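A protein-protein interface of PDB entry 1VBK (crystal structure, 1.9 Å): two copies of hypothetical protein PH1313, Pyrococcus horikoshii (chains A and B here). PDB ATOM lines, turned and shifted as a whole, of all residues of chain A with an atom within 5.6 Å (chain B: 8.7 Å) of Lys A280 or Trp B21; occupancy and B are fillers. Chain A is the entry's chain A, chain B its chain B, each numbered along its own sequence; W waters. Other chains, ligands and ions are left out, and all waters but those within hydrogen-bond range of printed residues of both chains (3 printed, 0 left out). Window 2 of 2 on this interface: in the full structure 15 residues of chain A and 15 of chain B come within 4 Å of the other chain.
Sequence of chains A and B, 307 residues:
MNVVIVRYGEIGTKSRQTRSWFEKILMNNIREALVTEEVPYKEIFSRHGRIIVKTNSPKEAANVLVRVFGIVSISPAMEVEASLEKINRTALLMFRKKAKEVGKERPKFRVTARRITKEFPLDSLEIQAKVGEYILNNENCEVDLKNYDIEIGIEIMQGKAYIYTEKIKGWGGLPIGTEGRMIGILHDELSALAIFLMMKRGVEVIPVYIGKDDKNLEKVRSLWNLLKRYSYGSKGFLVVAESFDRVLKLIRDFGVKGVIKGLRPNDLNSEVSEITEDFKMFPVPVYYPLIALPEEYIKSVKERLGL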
ATOM      1  N   LEU A 248      12.348  16.627  15.751  1.00  0.00           N
ATOM      2  CA  LEU A 248      12.297  16.913  14.321  1.00  0.00           C
ATOM      3  C   LEU A 248      13.145  15.885  13.578  1.00  0.00           C
ATOM      4  O   LEU A 248      12.767  15.422  12.506  1.00  0.00           O
ATOM      5  CB  LEU A 248      12.811  18.326  14.031  1.00  0.00           C
ATOM      6  CG  LEU A 248      11.937  19.464  14.571  1.00  0.00           C
ATOM      7  CD1 LEU A 248      12.653  20.802  14.395  1.00  0.00           C
ATOM      8  CD2 LEU A 248      10.599  19.464  13.849  1.00  0.00           C
ATOM      9  N   ILE A 275      -2.746  25.340  19.623  1.00  0.00           N
ATOM     10  CA  ILE A 275      -3.030  24.686  18.351  1.00  0.00           C
ATOM     11  C   ILE A 275      -2.327  25.407  17.197  1.00  0.00           C
ATOM     12  O   ILE A 275      -1.727  24.769  16.329  1.00  0.00           O
ATOM     13  CB  ILE A 275      -4.558  24.629  18.078  1.00  0.00           C
ATOM     14  CG1 ILE A 275      -5.219  23.653  19.056  1.00  0.00           C
ATOM     15  CG2 ILE A 275      -4.824  24.192  16.643  1.00  0.00           C
ATOM     16  CD1 ILE A 275      -6.730  23.613  18.961  1.00  0.00           C
ATOM     17  N   THR A 276      -2.398  26.735  17.192  1.00  0.00           N
ATOM     18  CA  THR A 276      -1.754  27.522  16.144  1.00  0.00           C
ATOM     19  C   THR A 276      -0.231  27.425  16.271  1.00  0.00           C
ATOM     20  O   THR A 276       0.485  27.365  15.269  1.00  0.00           O
ATOM     21  CB  THR A 276      -2.192  28.997  16.221  1.00  0.00           C
ATOM     22  OG1 THR A 276      -1.953  29.501  17.542  1.00  0.00           O
ATOM     23  CG2 THR A 276      -3.683  29.119  15.906  1.00  0.00           C
ATOM     24  N   GLU A 277       0.256  27.409  17.508  1.00  0.00           N
ATOM     25  CA  GLU A 277       1.688  27.290  17.770  1.00  0.00           C
ATOM     26  C   GLU A 277       2.158  25.910  17.302  1.00  0.00           C
ATOM     27  O   GLU A 277       3.203  25.788  16.660  1.00  0.00           O
ATOM     28  CB  GLU A 277       1.964  27.472  19.267  1.00  0.00           C
ATOM     29  CG  GLU A 277       1.995  28.929  19.718  1.00  0.00           C
ATOM     30  CD  GLU A 277       1.788  29.090  21.213  1.00  0.00           C
ATOM     31  OE1 GLU A 277       2.146  28.164  21.971  1.00  0.00           O
ATOM     32  OE2 GLU A 277       1.276  30.151  21.636  1.00  0.00           O
ATOM     33  N   ASP A 278       1.373  24.881  17.625  1.00  0.00           N
ATOM     34  CA  ASP A 278       1.673  23.504  17.227  1.00  0.00           C
ATOM     35  C   ASP A 278       1.784  23.427  15.717  1.00  0.00           C
ATOM     36  O   ASP A 278       2.673  22.774  15.170  1.00  0.00           O
ATOM     37  CB  ASP A 278       0.559  22.553  17.673  1.00  0.00           C
ATOM     38  CG  ASP A 278       0.767  22.012  19.067  1.00  0.00           C
ATOM     39  OD1 ASP A 278      -0.112  21.264  19.542  1.00  0.00           O
ATOM     40  OD2 ASP A 278       1.806  22.324  19.685  1.00  0.00           O
ATOM     41  N   PHE A 279       0.857  24.093  15.043  1.00  0.00           N
ATOM     42  CA  PHE A 279       0.845  24.101  13.594  1.00  0.00           C
ATOM     43  C   PHE A 279       2.155  24.648  13.033  1.00  0.00           C
ATOM     44  O   PHE A 279       2.600  24.241  11.957  1.00  0.00           O
ATOM     45  CB  PHE A 279      -0.322  24.946  13.083  1.00  0.00           C
ATOM     46  CG  PHE A 279      -0.398  25.013  11.594  1.00  0.00           C
ATOM     47  CD1 PHE A 279      -0.926  23.951  10.866  1.00  0.00           C
ATOM     48  CD2 PHE A 279       0.102  26.115  10.908  1.00  0.00           C
ATOM     49  CE1 PHE A 279      -0.952  23.985   9.472  1.00  0.00           C
ATOM     50  CE2 PHE A 279       0.081  26.158   9.514  1.00  0.00           C
ATOM     51  CZ  PHE A 279      -0.448  25.090   8.797  1.00  0.00           C
ATOM     52  N   LYS A 280       2.776  25.567  13.762  1.00  0.00           N
ATOM     53  CA  LYS A 280       4.022  26.166  13.304  1.00  0.00           C
ATOM     54  C   LYS A 280       5.293  25.429  13.715  1.00  0.00           C
ATOM     55  O   LYS A 280       6.275  25.444  12.978  1.00  0.00           O
ATOM     56  CB  LYS A 280       4.116  27.618  13.781  1.00  0.00           C
ATOM     57  CG  LYS A 280       3.066  28.546  13.184  1.00  0.00           C
ATOM     58  CD  LYS A 280       3.175  29.939  13.780  1.00  0.00           C
ATOM     59  CE  LYS A 280       2.154  30.888  13.177  1.00  0.00           C
ATOM     60  NZ  LYS A 280       2.174  32.214  13.864  1.00  0.00           N
ATOM     61  N   MET A 281       5.292  24.786  14.881  1.00  0.00           N
ATOM     62  CA  MET A 281       6.497  24.097  15.324  1.00  0.00           C
ATOM     63  C   MET A 281       6.732  22.718  14.709  1.00  0.00           C
ATOM     64  O   MET A 281       7.859  22.224  14.718  1.00  0.00           O
ATOM     65  CB  MET A 281       6.545  24.020  16.866  1.00  0.00           C
ATOM     66  CG  MET A 281       5.368  23.353  17.558  1.00  0.00           C
ATOM     67  SD  MET A 281       5.444  23.542  19.383  1.00  0.00           S
ATOM     68  CE  MET A 281       6.684  22.335  19.811  1.00  0.00           C
ATOM     69  N   PHE A 282       5.684  22.105  14.164  1.00  0.00           N
ATOM     70  CA  PHE A 282       5.803  20.787  13.542  1.00  0.00           C
ATOM     71  C   PHE A 282       5.635  20.872  12.024  1.00  0.00           C
ATOM     72  O   PHE A 282       4.756  21.574  11.531  1.00  0.00           O
ATOM     73  CB  PHE A 282       4.741  19.836  14.106  1.00  0.00           C
ATOM     74  CG  PHE A 282       4.959  19.453  15.537  1.00  0.00           C
ATOM     75  CD1 PHE A 282       5.936  18.519  15.877  1.00  0.00           C
ATOM     76  CD2 PHE A 282       4.181  20.011  16.544  1.00  0.00           C
ATOM     77  CE1 PHE A 282       6.133  18.147  17.200  1.00  0.00           C
ATOM     78  CE2 PHE A 282       4.370  19.646  17.875  1.00  0.00           C
ATOM     79  CZ  PHE A 282       5.351  18.708  18.203  1.00  0.00           C
ATOM     80  N   PRO A 283       6.479  20.150  11.267  1.00  0.00           N
ATOM     81  CA  PRO A 283       6.447  20.122   9.801  1.00  0.00           C
ATOM     82  C   PRO A 283       5.354  19.204   9.250  1.00  0.00           C
ATOM     83  O   PRO A 283       5.166  19.106   8.035  1.00  0.00           O
ATOM     84  CB  PRO A 283       7.837  19.624   9.446  1.00  0.00           C
ATOM     85  CG  PRO A 283       8.095  18.635  10.538  1.00  0.00           C
ATOM     86  CD  PRO A 283       7.635  19.386  11.771  1.00  0.00           C
ATOM     87  N   SER B  15       3.571  24.713  -3.603  1.00  0.00           N
ATOM     88  CA  SER B  15       4.000  23.767  -2.579  1.00  0.00           C
ATOM     89  C   SER B  15       2.897  23.482  -1.570  1.00  0.00           C
ATOM     90  O   SER B  15       2.076  24.347  -1.276  1.00  0.00           O
ATOM     91  CB  SER B  15       5.226  24.326  -1.848  1.00  0.00           C
ATOM     92  OG  SER B  15       5.543  23.556  -0.701  1.00  0.00           O
ATOM     93  N   ARG B  16       2.885  22.261  -1.039  1.00  0.00           N
ATOM     94  CA  ARG B  16       1.897  21.874  -0.042  1.00  0.00           C
ATOM     95  C   ARG B  16       2.415  22.310   1.327  1.00  0.00           C
ATOM     96  O   ARG B  16       1.719  22.210   2.337  1.00  0.00           O
ATOM     97  CB  ARG B  16       1.692  20.356  -0.052  1.00  0.00           C
ATOM     98  CG  ARG B  16       2.870  19.562   0.502  1.00  0.00           C
ATOM     99  CD  ARG B  16       2.576  18.067   0.510  1.00  0.00           C
ATOM    100  NE  ARG B  16       3.632  17.300   1.167  1.00  0.00           N
ATOM    101  CZ  ARG B  16       3.679  15.972   1.204  1.00  0.00           C
ATOM    102  NH1 ARG B  16       2.728  15.256   0.618  1.00  0.00           N
ATOM    103  NH2 ARG B  16       4.675  15.359   1.831  1.00  0.00           N
ATOM    104  N   GLN B  17       3.648  22.804   1.341  1.00  0.00           N
ATOM    105  CA  GLN B  17       4.307  23.254   2.562  1.00  0.00           C
ATOM    106  C   GLN B  17       4.007  24.729   2.822  1.00  0.00           C
ATOM    107  O   GLN B  17       3.810  25.494   1.880  1.00  0.00           O
ATOM    108  CB  GLN B  17       5.819  23.073   2.405  1.00  0.00           C
ATOM    109  CG  GLN B  17       6.561  22.735   3.674  1.00  0.00           C
ATOM    110  CD  GLN B  17       6.219  21.354   4.181  1.00  0.00           C
ATOM    111  OE1 GLN B  17       5.887  21.180   5.353  1.00  0.00           O
ATOM    112  NE2 GLN B  17       6.290  20.363   3.300  1.00  0.00           N
ATOM    113  N   THR B  18       3.969  25.132   4.090  1.00  0.00           N
ATOM    114  CA  THR B  18       3.730  26.537   4.396  1.00  0.00           C
ATOM    115  C   THR B  18       4.997  27.254   3.961  1.00  0.00           C
ATOM    116  O   THR B  18       6.015  26.614   3.694  1.00  0.00           O
ATOM    117  CB  THR B  18       3.533  26.802   5.907  1.00  0.00           C
ATOM    118  OG1 THR B  18       4.785  26.651   6.588  1.00  0.00           O
ATOM    119  CG2 THR B  18       2.513  25.844   6.494  1.00  0.00           C
ATOM    120  N   ARG B  19       4.940  28.576   3.894  1.00  0.00           N
ATOM    121  CA  ARG B  19       6.094  29.366   3.486  1.00  0.00           C
ATOM    122  C   ARG B  19       7.286  29.158   4.420  1.00  0.00           C
ATOM    123  O   ARG B  19       8.413  28.963   3.968  1.00  0.00           O
ATOM    124  CB  ARG B  19       5.718  30.845   3.450  1.00  0.00           C
ATOM    125  CG  ARG B  19       6.858  31.779   3.088  1.00  0.00           C
ATOM    126  CD  ARG B  19       6.429  33.230   3.254  1.00  0.00           C
ATOM    127  NE  ARG B  19       7.551  34.155   3.128  1.00  0.00           N
ATOM    128  CZ  ARG B  19       7.471  35.462   3.364  1.00  0.00           C
ATOM    129  NH1 ARG B  19       6.318  36.003   3.739  1.00  0.00           N
ATOM    130  NH2 ARG B  19       8.547  36.227   3.232  1.00  0.00           N
ATOM    131  N   SER B  20       7.035  29.205   5.725  1.00  0.00           N
ATOM    132  CA  SER B  20       8.104  29.035   6.700  1.00  0.00           C
ATOM    133  C   SER B  20       8.793  27.669   6.605  1.00  0.00           C
ATOM    134  O   SER B  20      10.017  27.586   6.690  1.00  0.00           O
ATOM    135  CB  SER B  20       7.567  29.256   8.117  1.00  0.00           C
ATOM    136  OG  SER B  20       6.457  28.413   8.369  1.00  0.00           O
ATOM    137  N   TRP B  21       8.025  26.597   6.433  1.00  0.00           N
ATOM    138  CA  TRP B  21       8.650  25.286   6.325  1.00  0.00           C
ATOM    139  C   TRP B  21       9.397  25.127   5.009  1.00  0.00           C
ATOM    140  O   TRP B  21      10.442  24.480   4.963  1.00  0.00           O
ATOM    141  CB  TRP B  21       7.620  24.172   6.510  1.00  0.00           C
ATOM    142  CG  TRP B  21       7.350  23.940   7.960  1.00  0.00           C
ATOM    143  CD1 TRP B  21       6.203  24.232   8.645  1.00  0.00           C
ATOM    144  CD2 TRP B  21       8.281  23.445   8.928  1.00  0.00           C
ATOM    145  NE1 TRP B  21       6.366  23.953   9.981  1.00  0.00           N
ATOM    146  CE2 TRP B  21       7.632  23.469  10.183  1.00  0.00           C
ATOM    147  CE3 TRP B  21       9.603  22.983   8.856  1.00  0.00           C
ATOM    148  CZ2 TRP B  21       8.258  23.051  11.360  1.00  0.00           C
ATOM    149  CZ3 TRP B  21      10.230  22.564  10.031  1.00  0.00           C
ATOM    150  CH2 TRP B  21       9.554  22.603  11.265  1.00  0.00           C
ATOM    151  N   PHE B  22       8.866  25.724   3.946  1.00  0.00           N
ATOM    152  CA  PHE B  22       9.515  25.674   2.637  1.00  0.00           C
ATOM    153  C   PHE B  22      10.912  26.282   2.789  1.00  0.00           C
ATOM    154  O   PHE B  22      11.901  25.719   2.316  1.00  0.00           O
ATOM    155  CB  PHE B  22       8.688  26.469   1.611  1.00  0.00           C
ATOM    156  CG  PHE B  22       9.336  26.598   0.244  1.00  0.00           C
ATOM    157  CD1 PHE B  22      10.460  27.398   0.056  1.00  0.00           C
ATOM    158  CD2 PHE B  22       8.801  25.934  -0.856  1.00  0.00           C
ATOM    159  CE1 PHE B  22      11.044  27.538  -1.205  1.00  0.00           C
ATOM    160  CE2 PHE B  22       9.375  26.067  -2.125  1.00  0.00           C
ATOM    161  CZ  PHE B  22      10.497  26.869  -2.298  1.00  0.00           C
ATOM    162  N   GLU B  23      10.989  27.426   3.466  1.00  0.00           N
ATOM    163  CA  GLU B  23      12.266  28.106   3.672  1.00  0.00           C
ATOM    164  C   GLU B  23      13.207  27.326   4.591  1.00  0.00           C
ATOM    165  O   GLU B  23      14.404  27.216   4.311  1.00  0.00           O
ATOM    166  CB  GLU B  23      12.021  29.522   4.214  1.00  0.00           C
ATOM    167  CG  GLU B  23      11.274  30.402   3.211  1.00  0.00           C
ATOM    168  CD  GLU B  23      10.829  31.738   3.777  1.00  0.00           C
ATOM    169  OE1 GLU B  23      10.382  31.785   4.943  1.00  0.00           O
ATOM    170  OE2 GLU B  23      10.915  32.744   3.044  1.00  0.00           O
ATOM    171  N   LYS B  24      12.680  26.774   5.681  1.00  0.00           N
ATOM    172  CA  LYS B  24      13.524  26.002   6.590  1.00  0.00           C
ATOM    173  C   LYS B  24      14.115  24.765   5.908  1.00  0.00           C
ATOM    174  O   LYS B  24      15.291  24.448   6.091  1.00  0.00           O
ATOM    175  CB  LYS B  24      12.733  25.578   7.827  1.00  0.00           C
ATOM    176  CG  LYS B  24      12.478  26.706   8.806  1.00  0.00           C
ATOM    177  CD  LYS B  24      11.643  26.222   9.978  1.00  0.00           C
ATOM    178  CE  LYS B  24      11.415  27.336  10.988  1.00  0.00           C
ATOM    179  NZ  LYS B  24      10.518  26.865  12.074  1.00  0.00           N
ATOM    180  N   ILE B  25      13.297  24.064   5.130  1.00  0.00           N
ATOM    181  CA  ILE B  25      13.757  22.868   4.428  1.00  0.00           C
ATOM    182  C   ILE B  25      14.772  23.253   3.355  1.00  0.00           C
ATOM    183  O   ILE B  25      15.798  22.590   3.192  1.00  0.00           O
ATOM    184  CB  ILE B  25      12.564  22.113   3.791  1.00  0.00           C
ATOM    185  CG1 ILE B  25      11.662  21.561   4.901  1.00  0.00           C
ATOM    186  CG2 ILE B  25      13.059  20.969   2.922  1.00  0.00           C
ATOM    187  CD1 ILE B  25      10.333  21.057   4.408  1.00  0.00           C
ATOM    188  N   LEU B  26      14.499  24.337   2.633  1.00  0.00           N
ATOM    189  CA  LEU B  26      15.423  24.792   1.602  1.00  0.00           C
ATOM    190  C   LEU B  26      16.765  25.204   2.212  1.00  0.00           C
ATOM    191  O   LEU B  26      17.813  24.906   1.647  1.00  0.00           O
ATOM    192  CB  LEU B  26      14.820  25.963   0.810  1.00  0.00           C
ATOM    193  CG  LEU B  26      15.713  26.570  -0.278  1.00  0.00           C
ATOM    194  CD1 LEU B  26      16.177  25.484  -1.261  1.00  0.00           C
ATOM    195  CD2 LEU B  26      14.929  27.651  -1.017  1.00  0.00           C
ATOM    196  N   MET B  27      16.740  25.888   3.354  1.00  0.00           N
ATOM    197  CA  MET B  27      17.988  26.294   4.006  1.00  0.00           C
ATOM    198  C   MET B  27      18.757  25.053   4.472  1.00  0.00           C
ATOM    199  O   MET B  27      19.992  25.029   4.439  1.00  0.00           O
ATOM    200  CB  MET B  27      17.717  27.224   5.197  1.00  0.00           C
ATOM    201  CG  MET B  27      17.318  28.645   4.791  1.00  0.00           C
ATOM    202  SD  MET B  27      17.275  29.808   6.178  1.00  0.00           S
ATOM    203  CE  MET B  27      15.776  29.300   6.978  1.00  0.00           C
ATOM    204  N   ASN B  28      18.025  24.033   4.910  1.00  0.00           N
ATOM    205  CA  ASN B  28      18.643  22.782   5.345  1.00  0.00           C
ATOM    206  C   ASN B  28      19.380  22.147   4.169  1.00  0.00           C
ATOM    207  O   ASN B  28      20.507  21.672   4.314  1.00  0.00           O
ATOM    208  CB  ASN B  28      17.579  21.796   5.848  1.00  0.00           C
ATOM    209  CG  ASN B  28      18.144  20.402   6.099  1.00  0.00           C
ATOM    210  OD1 ASN B  28      18.709  20.133   7.156  1.00  0.00           O
ATOM    211  ND2 ASN B  28      18.000  19.513   5.118  1.00  0.00           N
ATOM    212  N   ASN B  29      18.729  22.135   3.007  1.00  0.00           N
ATOM    213  CA  ASN B  29      19.306  21.543   1.804  1.00  0.00           C
ATOM    214  C   ASN B  29      20.502  22.339   1.299  1.00  0.00           C
ATOM    215  O   ASN B  29      21.484  21.766   0.820  1.00  0.00           O
ATOM    216  CB  ASN B  29      18.230  21.414   0.715  1.00  0.00           C
ATOM    217  CG  ASN B  29      17.122  20.442   1.113  1.00  0.00           C
ATOM    218  OD1 ASN B  29      17.204  19.787   2.153  1.00  0.00           O
ATOM    219  ND2 ASN B  29      16.086  20.345   0.289  1.00  0.00           N
ATOM    220  N   PRO B 175      11.821  22.260  -3.024  1.00  0.00           N
ATOM    221  CA  PRO B 175      12.906  21.759  -2.170  1.00  0.00           C
ATOM    222  C   PRO B 175      12.733  20.287  -1.816  1.00  0.00           C
ATOM    223  O   PRO B 175      11.628  19.842  -1.484  1.00  0.00           O
ATOM    224  CB  PRO B 175      12.822  22.655  -0.937  1.00  0.00           C
ATOM    225  CG  PRO B 175      12.169  23.926  -1.465  1.00  0.00           C
ATOM    226  CD  PRO B 175      11.114  23.376  -2.375  1.00  0.00           C
ATOM    227  N   ILE B 176      13.827  19.532  -1.880  1.00  0.00           N
ATOM    228  CA  ILE B 176      13.771  18.114  -1.555  1.00  0.00           C
ATOM    229  C   ILE B 176      13.304  17.916  -0.120  1.00  0.00           C
ATOM    230  O   ILE B 176      13.833  18.523   0.814  1.00  0.00           O
ATOM    231  CB  ILE B 176      15.144  17.430  -1.728  1.00  0.00           C
ATOM    232  CG1 ILE B 176      15.554  17.462  -3.202  1.00  0.00           C
ATOM    233  CG2 ILE B 176      15.066  15.976  -1.244  1.00  0.00           C
ATOM    234  CD1 ILE B 176      16.847  16.748  -3.491  1.00  0.00           C
ATOM    235  N   GLY B 177      12.309  17.053   0.048  1.00  0.00           N
ATOM    236  CA  GLY B 177      11.788  16.796   1.374  1.00  0.00           C
ATOM    237  C   GLY B 177      10.492  17.530   1.675  1.00  0.00           C
ATOM    238  O   GLY B 177       9.871  17.266   2.699  1.00  0.00           O
ATOM    239  N   THR B 178      10.073  18.444   0.803  1.00  0.00           N
ATOM    240  CA  THR B 178       8.830  19.174   1.046  1.00  0.00           C
ATOM    241  C   THR B 178       7.603  18.388   0.600  1.00  0.00           C
ATOM    242  O   THR B 178       6.486  18.681   1.029  1.00  0.00           O
ATOM    243  CB  THR B 178       8.810  20.550   0.336  1.00  0.00           C
ATOM    244  OG1 THR B 178       9.089  20.379  -1.060  1.00  0.00           O
ATOM    245  CG2 THR B 178       9.836  21.493   0.963  1.00  0.00           C
HETATM  246  O   HOH W   1       8.613  26.552  13.698  1.00  0.00           O
HETATM  247  O   HOH W   2       7.040  27.322  10.861  1.00  0.00           O
HETATM  248  O   HOH W   3       3.319  22.479   9.279  1.00  0.00           O
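O of Lys A280 is in hydrogen-bond range of NE1 of Trp B21 (3.3 Å). NE1 of Trp B21 is in hydrogen-bond range of O of Phe A282 (3.3 Å). O of Pro A283 sits close to OE1 of Gln B17 (3.5 Å).
OG of Ser B15 sits at hydrogen-bond distance from N of Gln B17 (2.9 Å). The side-chain amide nitrogen of Gln B17 sits at hydrogen-bond distance from the backbone carbonyl oxygen of Thr B178. The side-chain hydroxyl (OG1) of Thr B18 sits at hydrogen-bond distance from the side-chain hydroxyl (OG) of Ser B20 (3.0 Å). The backbone NH (N) of Trp B21 lies within hydrogen-bond range of the side-chain hydroxyl (OG1) of Thr B18 (3.2 Å).
Phe A279 touches Thr B18 (CZ to CG2, 3.8 Å). Met A281 touches Trp B21. Pro A283 touches Trp B21.
Trp B21 touches just these residues of chain A: Lys A280 (3.3 Å), Met A281 (3.5 Å), Phe A282 (3.3 Å) and Pro A283 (3.4 Å). Printed residues of chain B within 4 Å of Phe A279: Thr B18. Printed residues of chain B within 4 Å of Phe A282: Trp B21. Printed residues of chain A within 4 Å of Thr B18: Phe A279 (3.8 Å). Of the printed residues of chain A, Gln B17 touches Pro A283. Thr A276 touches none of the printed residues of chain B. The nearest residue of chain B that does not touch Lys A280 is Lys B24 (4.6 Å).
Of the 10 printed residues of chain A, 5 touch a printed residue of chain B. Of the 19 printed residues of chain B, 3 touch a printed residue of chain A. Among the printed residues, no Asp or Glu carboxylate lies within 4 Å of a Lys or Arg side-chain nitrogen of the other chain.
No position is printed for both chains. Of the 6 pairs that touch across the chains among the printed residues, none has its exchanged pair printed and touching as well.
Water W1 lies within hydrogen-bond range of NZ of Lys B24 and O of Lys A280. Water W2 lies within hydrogen-bond range of the side-chain hydroxyl (OG) of Ser B20 (2.8 Å) and the backbone carbonyl oxygen (O) of Lys A280 (2.9 Å). Water W3 lies within hydrogen-bond range of O of Phe A282 (2.8 Å), O of Phe A279 (3.3 Å) and NE1 of Trp B21 (3.5 Å).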
